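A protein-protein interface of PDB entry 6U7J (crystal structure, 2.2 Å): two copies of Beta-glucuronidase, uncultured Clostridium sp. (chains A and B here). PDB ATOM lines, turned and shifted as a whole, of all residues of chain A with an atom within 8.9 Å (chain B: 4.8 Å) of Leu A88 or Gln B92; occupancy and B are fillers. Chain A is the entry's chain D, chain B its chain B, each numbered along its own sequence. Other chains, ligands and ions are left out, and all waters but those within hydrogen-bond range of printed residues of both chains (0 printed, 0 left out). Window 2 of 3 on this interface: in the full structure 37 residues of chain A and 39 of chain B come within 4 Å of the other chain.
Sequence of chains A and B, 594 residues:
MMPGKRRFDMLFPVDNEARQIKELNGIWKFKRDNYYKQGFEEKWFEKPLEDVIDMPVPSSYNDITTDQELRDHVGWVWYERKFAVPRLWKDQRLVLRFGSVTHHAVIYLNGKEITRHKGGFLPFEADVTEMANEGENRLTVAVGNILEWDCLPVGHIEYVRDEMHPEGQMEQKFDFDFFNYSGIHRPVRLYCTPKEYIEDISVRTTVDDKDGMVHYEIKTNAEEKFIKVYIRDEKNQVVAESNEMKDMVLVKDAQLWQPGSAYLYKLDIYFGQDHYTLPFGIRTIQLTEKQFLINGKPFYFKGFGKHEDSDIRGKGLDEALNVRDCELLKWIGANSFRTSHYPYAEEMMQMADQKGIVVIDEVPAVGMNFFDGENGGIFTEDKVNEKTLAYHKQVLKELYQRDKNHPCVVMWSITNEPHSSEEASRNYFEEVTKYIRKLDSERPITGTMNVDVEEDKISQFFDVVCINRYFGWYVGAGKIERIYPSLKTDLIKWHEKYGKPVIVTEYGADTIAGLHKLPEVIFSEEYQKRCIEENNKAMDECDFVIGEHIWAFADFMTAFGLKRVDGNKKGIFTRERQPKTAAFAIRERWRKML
The side-chain amide oxygen (OE1) of Gln A20 lies within hydrogen-bond range of the indole nitrogen (NE1) of Trp B89 (3.4 Å).
NE1 of Trp A89 sits at hydrogen-bond distance from OE1 of Gln A20.
The backbone NH (N) of Cys A192 is in hydrogen-bond range of the backbone carbonyl oxygen (O) of Gln A20, at 3.0 Å.
CB of Ala B18 touches NH2 of Arg A87 (3.7 Å).
Leu B88 touches Leu A88.
CD2 of Leu A88 touches OE1 of Gln B92, 3.6 Å away.
Leu B88 touches Gln A92 (CD1 to CD, 3.5 Å).
Printed residues of chain B within 4 Å of Gln A20: Trp B89.
Printed residues of chain B within 4 Å of Arg A87: Ala B18 (3.7 Å).
Of chain B, only Leu B88 and Gln B92 come within 4 Å of Leu A88.
Of the printed residues of chain B, Gln A92 touches Leu B88.
Printed residues of chain A within 4 Å of Leu B88: Leu A88 and Gln A92.
Of the printed residues of chain A, Trp B89 touches Gln A20.
Cys B192 touches none of the printed residues of chain A.
Lys B195 touches none of the printed residues of chain A.
The nearest printed residue of chain B that does not touch Arg A87 is Pro B194 (4.7 Å).
Printed residues of chain A that touch a printed residue of chain B: Gln A20, Arg A87, Leu A88 and Gln A92.
Hydrophobic or aromatic side chains of chain A that line the printed part of chain B: Leu A88.
Of the 13 printed residues of chain B, 4 touch a printed residue of chain A.
Among the printed residues, 5 pairs touch across the chains.
Leu B88 touches its own counterpart, Leu A88.
Leu A88 touches Gln B92, and with the chains exchanged Gln A92 touches Leu B88.
7 positions are printed for both chains.
Of the 5 pairs that touch across the chains among the printed residues, 3 have their exchanged pair printed and touching as well.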
ATOM      1  N   GLN A  20       6.146  15.192  13.285  1.00  0.00           N
ATOM      2  CA  GLN A  20       5.434  16.430  12.996  1.00  0.00           C
ATOM      3  C   GLN A  20       4.018  16.131  12.513  1.00  0.00           C
ATOM      4  O   GLN A  20       3.800  15.165  11.774  1.00  0.00           O
ATOM      5  CB  GLN A  20       6.177  17.252  11.943  1.00  0.00           C
ATOM      6  CG  GLN A  20       5.685  18.683  11.808  1.00  0.00           C
ATOM      7  CD  GLN A  20       6.252  19.349  10.577  1.00  0.00           C
ATOM      8  OE1 GLN A  20       7.415  19.139  10.224  1.00  0.00           O
ATOM      9  NE2 GLN A  20       5.428  20.138   9.899  1.00  0.00           N
ATOM     10  N   VAL A  85       2.393  17.836   0.548  1.00  0.00           N
ATOM     11  CA  VAL A  85       3.565  17.232   1.170  1.00  0.00           C
ATOM     12  C   VAL A  85       4.760  18.126   0.862  1.00  0.00           C
ATOM     13  O   VAL A  85       5.122  18.290  -0.316  1.00  0.00           O
ATOM     14  CB  VAL A  85       3.805  15.794   0.683  1.00  0.00           C
ATOM     15  CG1 VAL A  85       5.045  15.198   1.357  1.00  0.00           C
ATOM     16  CG2 VAL A  85       2.601  14.933   0.955  1.00  0.00           C
ATOM     17  N   PRO A  86       5.384  18.734   1.866  1.00  0.00           N
ATOM     18  CA  PRO A  86       6.519  19.630   1.598  1.00  0.00           C
ATOM     19  C   PRO A  86       7.764  18.862   1.164  1.00  0.00           C
ATOM     20  O   PRO A  86       7.956  17.693   1.495  1.00  0.00           O
ATOM     21  CB  PRO A  86       6.746  20.325   2.944  1.00  0.00           C
ATOM     22  CG  PRO A  86       6.225  19.325   3.973  1.00  0.00           C
ATOM     23  CD  PRO A  86       5.101  18.588   3.308  1.00  0.00           C
ATOM     24  N   ARG A  87       8.606  19.548   0.394  1.00  0.00           N
ATOM     25  CA  ARG A  87       9.929  19.013   0.046  1.00  0.00           C
ATOM     26  C   ARG A  87      10.670  18.530   1.293  1.00  0.00           C
ATOM     27  O   ARG A  87      11.323  17.496   1.257  1.00  0.00           O
ATOM     28  CB  ARG A  87      10.770  20.084  -0.662  1.00  0.00           C
ATOM     29  CG  ARG A  87      10.644  20.112  -2.166  1.00  0.00           C
ATOM     30  CD  ARG A  87      11.665  21.068  -2.784  1.00  0.00           C
ATOM     31  NE  ARG A  87      11.679  22.372  -2.124  1.00  0.00           N
ATOM     32  CZ  ARG A  87      11.266  23.496  -2.706  1.00  0.00           C
ATOM     33  NH1 ARG A  87      10.812  23.471  -3.954  1.00  0.00           N
ATOM     34  NH2 ARG A  87      11.306  24.644  -2.042  1.00  0.00           N
ATOM     35  N   LEU A  88      10.537  19.249   2.411  1.00  0.00           N
ATOM     36  CA  LEU A  88      11.268  18.926   3.630  1.00  0.00           C
ATOM     37  C   LEU A  88      10.901  17.564   4.229  1.00  0.00           C
ATOM     38  O   LEU A  88      11.637  17.069   5.078  1.00  0.00           O
ATOM     39  CB  LEU A  88      11.040  20.017   4.680  1.00  0.00           C
ATOM     40  CG  LEU A  88      11.343  21.415   4.172  1.00  0.00           C
ATOM     41  CD1 LEU A  88      10.417  22.436   4.807  1.00  0.00           C
ATOM     42  CD2 LEU A  88      12.801  21.783   4.399  1.00  0.00           C
ATOM     43  N   TRP A  89       9.815  16.941   3.783  1.00  0.00           N
ATOM     44  CA  TRP A  89       9.396  15.642   4.296  1.00  0.00           C
ATOM     45  C   TRP A  89       9.879  14.479   3.414  1.00  0.00           C
ATOM     46  O   TRP A  89       9.342  13.366   3.503  1.00  0.00           O
ATOM     47  CB  TRP A  89       7.867  15.581   4.427  1.00  0.00           C
ATOM     48  CG  TRP A  89       7.280  16.253   5.655  1.00  0.00           C
ATOM     49  CD1 TRP A  89       7.902  17.139   6.493  1.00  0.00           C
ATOM     50  CD2 TRP A  89       5.948  16.091   6.166  1.00  0.00           C
ATOM     51  NE1 TRP A  89       7.036  17.528   7.498  1.00  0.00           N
ATOM     52  CE2 TRP A  89       5.835  16.897   7.319  1.00  0.00           C
ATOM     53  CE3 TRP A  89       4.843  15.336   5.764  1.00  0.00           C
ATOM     54  CZ2 TRP A  89       4.664  16.963   8.075  1.00  0.00           C
ATOM     55  CZ3 TRP A  89       3.678  15.407   6.519  1.00  0.00           C
ATOM     56  CH2 TRP A  89       3.603  16.209   7.665  1.00  0.00           C
ATOM     57  N   LYS A  90      10.886  14.714   2.572  1.00  0.00           N
ATOM     58  CA  LYS A  90      11.154  13.829   1.442  1.00  0.00           C
ATOM     59  C   LYS A  90      11.362  12.377   1.871  1.00  0.00           C
ATOM     60  O   LYS A  90      10.785  11.459   1.273  1.00  0.00           O
ATOM     61  CB  LYS A  90      12.363  14.313   0.639  1.00  0.00           C
ATOM     62  CG  LYS A  90      12.612  13.459  -0.605  1.00  0.00           C
ATOM     63  CD  LYS A  90      11.431  13.514  -1.597  1.00  0.00           C
ATOM     64  CE  LYS A  90      10.952  12.113  -2.035  1.00  0.00           C
ATOM     65  NZ  LYS A  90      10.000  11.476  -1.057  1.00  0.00           N
ATOM     66  N   ASP A  91      12.198  12.129   2.872  1.00  0.00           N
ATOM     67  CA  ASP A  91      12.537  10.738   3.164  1.00  0.00           C
ATOM     68  C   ASP A  91      11.881  10.221   4.441  1.00  0.00           C
ATOM     69  O   ASP A  91      12.394   9.303   5.084  1.00  0.00           O
ATOM     70  CB  ASP A  91      14.051  10.562   3.216  1.00  0.00           C
ATOM     71  CG  ASP A  91      14.673  10.618   1.836  1.00  0.00           C
ATOM     72  OD1 ASP A  91      14.373   9.712   1.023  1.00  0.00           O
ATOM     73  OD2 ASP A  91      15.429  11.577   1.557  1.00  0.00           O
ATOM     74  N   GLN A  92      10.735  10.777   4.806  1.00  0.00           N
ATOM     75  CA  GLN A  92      10.066  10.375   6.031  1.00  0.00           C
ATOM     76  C   GLN A  92       8.976   9.361   5.733  1.00  0.00           C
ATOM     77  O   GLN A  92       8.521   9.205   4.598  1.00  0.00           O
ATOM     78  CB  GLN A  92       9.468  11.586   6.750  1.00  0.00           C
ATOM     79  CG  GLN A  92      10.433  12.738   6.913  1.00  0.00           C
ATOM     80  CD  GLN A  92      11.716  12.317   7.607  1.00  0.00           C
ATOM     81  OE1 GLN A  92      11.725  12.023   8.806  1.00  0.00           O
ATOM     82  NE2 GLN A  92      12.811  12.288   6.852  1.00  0.00           N
ATOM     83  N   LEU A  94       5.126   8.629   6.065  1.00  0.00           N
ATOM     84  CA  LEU A  94       3.961   9.508   6.050  1.00  0.00           C
ATOM     85  C   LEU A  94       2.706   8.715   6.405  1.00  0.00           C
ATOM     86  O   LEU A  94       2.458   7.653   5.826  1.00  0.00           O
ATOM     87  CB  LEU A  94       3.802  10.176   4.676  1.00  0.00           C
ATOM     88  CG  LEU A  94       5.024  10.942   4.156  1.00  0.00           C
ATOM     89  CD1 LEU A  94       4.735  11.653   2.845  1.00  0.00           C
ATOM     90  CD2 LEU A  94       5.474  11.937   5.199  1.00  0.00           C
ATOM     91  N   GLU A 134       4.979  14.710  -3.517  1.00  0.00           N
ATOM     92  CA  GLU A 134       5.430  16.023  -3.088  1.00  0.00           C
ATOM     93  C   GLU A 134       4.527  17.089  -3.698  1.00  0.00           C
ATOM     94  O   GLU A 134       4.081  16.968  -4.839  1.00  0.00           O
ATOM     95  CB  GLU A 134       6.886  16.222  -3.511  1.00  0.00           C
ATOM     96  CG  GLU A 134       7.393  17.635  -3.422  1.00  0.00           C
ATOM     97  CD  GLU A 134       8.877  17.733  -3.766  1.00  0.00           C
ATOM     98  OE1 GLU A 134       9.677  16.967  -3.175  1.00  0.00           O
ATOM     99  OE2 GLU A 134       9.241  18.575  -4.621  1.00  0.00           O
ATOM    100  N   GLY A 135       4.214  18.121  -2.925  1.00  0.00           N
ATOM    101  CA  GLY A 135       3.241  19.085  -3.401  1.00  0.00           C
ATOM    102  C   GLY A 135       1.813  18.585  -3.233  1.00  0.00           C
ATOM    103  O   GLY A 135       1.495  17.816  -2.316  1.00  0.00           O
ATOM    104  N   CYS A 192       4.286  12.782  10.028  1.00  0.00           N
ATOM    105  CA  CYS A 192       5.483  12.084   9.627  1.00  0.00           C
ATOM    106  C   CYS A 192       6.220  11.529  10.844  1.00  0.00           C
ATOM    107  O   CYS A 192       6.069  12.011  11.979  1.00  0.00           O
ATOM    108  CB  CYS A 192       6.409  12.988   8.750  1.00  0.00           C
ATOM    109  SG  CYS A 192       7.074  14.461   9.539  1.00  0.00           S
ATOM    110  N   ALA B  18       6.869  24.136  -0.656  1.00  0.00           N
ATOM    111  CA  ALA B  18       7.905  25.037  -0.159  1.00  0.00           C
ATOM    112  C   ALA B  18       7.643  25.569   1.238  1.00  0.00           C
ATOM    113  O   ALA B  18       8.589  25.747   2.003  1.00  0.00           O
ATOM    114  CB  ALA B  18       8.062  26.232  -1.105  1.00  0.00           C
ATOM    115  N   LEU B  88      13.609  18.813  10.511  1.00  0.00           N
ATOM    116  CA  LEU B  88      13.425  19.012   9.078  1.00  0.00           C
ATOM    117  C   LEU B  88      13.164  20.464   8.681  1.00  0.00           C
ATOM    118  O   LEU B  88      13.143  20.758   7.484  1.00  0.00           O
ATOM    119  CB  LEU B  88      12.300  18.107   8.596  1.00  0.00           C
ATOM    120  CG  LEU B  88      12.672  16.649   8.886  1.00  0.00           C
ATOM    121  CD1 LEU B  88      11.541  15.703   8.597  1.00  0.00           C
ATOM    122  CD2 LEU B  88      13.907  16.263   8.078  1.00  0.00           C
ATOM    123  N   TRP B  89      12.980  21.375   9.631  1.00  0.00           N
ATOM    124  CA  TRP B  89      12.863  22.804   9.352  1.00  0.00           C
ATOM    125  C   TRP B  89      14.177  23.542   9.566  1.00  0.00           C
ATOM    126  O   TRP B  89      14.193  24.776   9.542  1.00  0.00           O
ATOM    127  CB  TRP B  89      11.776  23.439  10.238  1.00  0.00           C
ATOM    128  CG  TRP B  89      10.351  23.105   9.858  1.00  0.00           C
ATOM    129  CD1 TRP B  89       9.932  22.069   9.084  1.00  0.00           C
ATOM    130  CD2 TRP B  89       9.164  23.814  10.253  1.00  0.00           C
ATOM    131  NE1 TRP B  89       8.559  22.084   8.970  1.00  0.00           N
ATOM    132  CE2 TRP B  89       8.066  23.145   9.679  1.00  0.00           C
ATOM    133  CE3 TRP B  89       8.925  24.940  11.046  1.00  0.00           C
ATOM    134  CZ2 TRP B  89       6.746  23.570   9.861  1.00  0.00           C
ATOM    135  CZ3 TRP B  89       7.611  25.359  11.230  1.00  0.00           C
ATOM    136  CH2 TRP B  89       6.540  24.678  10.636  1.00  0.00           C
ATOM    137  N   LYS B  90      15.271  22.803   9.781  1.00  0.00           N
ATOM    138  CA  LYS B  90      16.605  23.281  10.141  1.00  0.00           C
ATOM    139  C   LYS B  90      16.998  24.641   9.571  1.00  0.00           C
ATOM    140  O   LYS B  90      17.349  25.556  10.330  1.00  0.00           O
ATOM    141  CB  LYS B  90      17.640  22.239   9.700  1.00  0.00           C
ATOM    142  CG  LYS B  90      19.046  22.509  10.196  1.00  0.00           C
ATOM    143  CD  LYS B  90      19.950  21.317   9.936  1.00  0.00           C
ATOM    144  CE  LYS B  90      20.444  21.312   8.496  1.00  0.00           C
ATOM    145  NZ  LYS B  90      20.434  19.947   7.901  1.00  0.00           N
ATOM    146  N   ASP B  91      16.958  24.794   8.245  1.00  0.00           N
ATOM    147  CA  ASP B  91      17.450  26.000   7.591  1.00  0.00           C
ATOM    148  C   ASP B  91      16.331  26.870   7.029  1.00  0.00           C
ATOM    149  O   ASP B  91      16.566  27.647   6.096  1.00  0.00           O
ATOM    150  CB  ASP B  91      18.431  25.623   6.479  1.00  0.00           C
ATOM    151  CG  ASP B  91      19.733  25.084   7.019  1.00  0.00           C
ATOM    152  OD1 ASP B  91      20.373  25.794   7.822  1.00  0.00           O
ATOM    153  OD2 ASP B  91      20.103  23.947   6.662  1.00  0.00           O
ATOM    154  N   GLN B  92      15.119  26.766   7.568  1.00  0.00           N
ATOM    155  CA  GLN B  92      14.027  27.552   7.020  1.00  0.00           C
ATOM    156  C   GLN B  92      13.841  28.848   7.807  1.00  0.00           C
ATOM    157  O   GLN B  92      14.306  28.997   8.939  1.00  0.00           O
ATOM    158  CB  GLN B  92      12.735  26.733   7.007  1.00  0.00           C
ATOM    159  CG  GLN B  92      12.861  25.375   6.329  1.00  0.00           C
ATOM    160  CD  GLN B  92      13.521  25.460   4.960  1.00  0.00           C
ATOM    161  OE1 GLN B  92      14.599  24.899   4.740  1.00  0.00           O
ATOM    162  NE2 GLN B  92      12.880  26.162   4.035  1.00  0.00           N
ATOM    163  N   ARG B  93      13.186  29.809   7.170  1.00  0.00           N
ATOM    164  CA  ARG B  93      12.655  30.951   7.899  1.00  0.00           C
ATOM    165  C   ARG B  93      11.497  30.482   8.779  1.00  0.00           C
ATOM    166  O   ARG B  93      10.630  29.731   8.321  1.00  0.00           O
ATOM    167  CB  ARG B  93      12.192  32.029   6.919  1.00  0.00           C
ATOM    168  CG  ARG B  93      11.768  33.329   7.579  1.00  0.00           C
ATOM    169  CD  ARG B  93      11.530  34.405   6.530  1.00  0.00           C
ATOM    170  NE  ARG B  93      10.549  35.399   6.958  1.00  0.00           N
ATOM    171  CZ  ARG B  93       9.278  35.424   6.559  1.00  0.00           C
ATOM    172  NH1 ARG B  93       8.822  34.500   5.721  1.00  0.00           N
ATOM    173  NH2 ARG B  93       8.459  36.378   6.993  1.00  0.00           N
ATOM    174  N   LEU B  94      11.506  30.883  10.049  1.00  0.00           N
ATOM    175  CA  LEU B  94      10.497  30.482  11.026  1.00  0.00           C
ATOM    176  C   LEU B  94       9.728  31.711  11.482  1.00  0.00           C
ATOM    177  O   LEU B  94      10.335  32.685  11.940  1.00  0.00           O
ATOM    178  CB  LEU B  94      11.129  29.790  12.238  1.00  0.00           C
ATOM    179  CG  LEU B  94      12.056  28.598  11.984  1.00  0.00           C
ATOM    180  CD1 LEU B  94      12.422  27.946  13.312  1.00  0.00           C
ATOM    181  CD2 LEU B  94      11.471  27.573  11.037  1.00  0.00           C
ATOM    182  N   THR B 129      13.332  32.861  13.474  1.00  0.00           N
ATOM    183  CA  THR B 129      14.328  31.995  12.841  1.00  0.00           C
ATOM    184  C   THR B 129      15.580  31.832  13.694  1.00  0.00           C
ATOM    185  O   THR B 129      16.103  30.724  13.833  1.00  0.00           O
ATOM    186  CB  THR B 129      14.715  32.553  11.471  1.00  0.00           C
ATOM    187  OG1 THR B 129      13.530  32.913  10.748  1.00  0.00           O
ATOM    188  CG2 THR B 129      15.515  31.524  10.687  1.00  0.00           C
ATOM    189  N   CYS B 192       6.817  27.972   8.167  1.00  0.00           N
ATOM    190  CA  CYS B 192       8.144  28.099   7.593  1.00  0.00           C
ATOM    191  C   CYS B 192       8.075  28.523   6.125  1.00  0.00           C
ATOM    192  O   CYS B 192       7.063  28.316   5.441  1.00  0.00           O
ATOM    193  CB  CYS B 192       8.978  26.788   7.768  1.00  0.00           C
ATOM    194  SG  CYS B 192       8.463  25.332   6.847  1.00  0.00           S
ATOM    195  N   THR B 193       9.128  29.206   5.674  1.00  0.00           N
ATOM    196  CA  THR B 193       9.368  29.561   4.279  1.00  0.00           C
ATOM    197  C   THR B 193      10.857  29.433   3.984  1.00  0.00           C
ATOM    198  O   THR B 193      11.684  29.380   4.907  1.00  0.00           O
ATOM    199  CB  THR B 193       8.933  30.993   3.916  1.00  0.00           C
ATOM    200  OG1 THR B 193       9.870  31.941   4.440  1.00  0.00           O
ATOM    201  CG2 THR B 193       7.502  31.337   4.389  1.00  0.00           C
ATOM    202  N   PRO B 194      11.233  29.385   2.701  1.00  0.00           N
ATOM    203  CA  PRO B 194      12.642  29.582   2.341  1.00  0.00           C
ATOM    204  C   PRO B 194      13.127  30.954   2.791  1.00  0.00           C
ATOM    205  O   PRO B 194      12.337  31.884   2.989  1.00  0.00           O
ATOM    206  CB  PRO B 194      12.643  29.464   0.810  1.00  0.00           C
ATOM    207  CG  PRO B 194      11.419  28.645   0.488  1.00  0.00           C
ATOM    208  CD  PRO B 194      10.407  29.032   1.527  1.00  0.00           C
ATOM    209  N   LYS B 195      14.454  31.077   2.955  1.00  0.00           N
ATOM    210  CA  LYS B 195      15.012  32.343   3.425  1.00  0.00           C
ATOM    211  C   LYS B 195      14.919  33.450   2.380  1.00  0.00           C
ATOM    212  O   LYS B 195      14.936  34.634   2.740  1.00  0.00           O
ATOM    213  CB  LYS B 195      16.461  32.152   3.869  1.00  0.00           C
ATOM    214  CG  LYS B 195      16.619  31.120   4.963  1.00  0.00           C
ATOM    215  CD  LYS B 195      17.534  31.599   6.075  1.00  0.00           C
ATOM    216  CE  LYS B 195      17.437  30.666   7.291  1.00  0.00           C
ATOM    217  NZ  LYS B 195      18.633  30.741   8.189  1.00  0.00           N
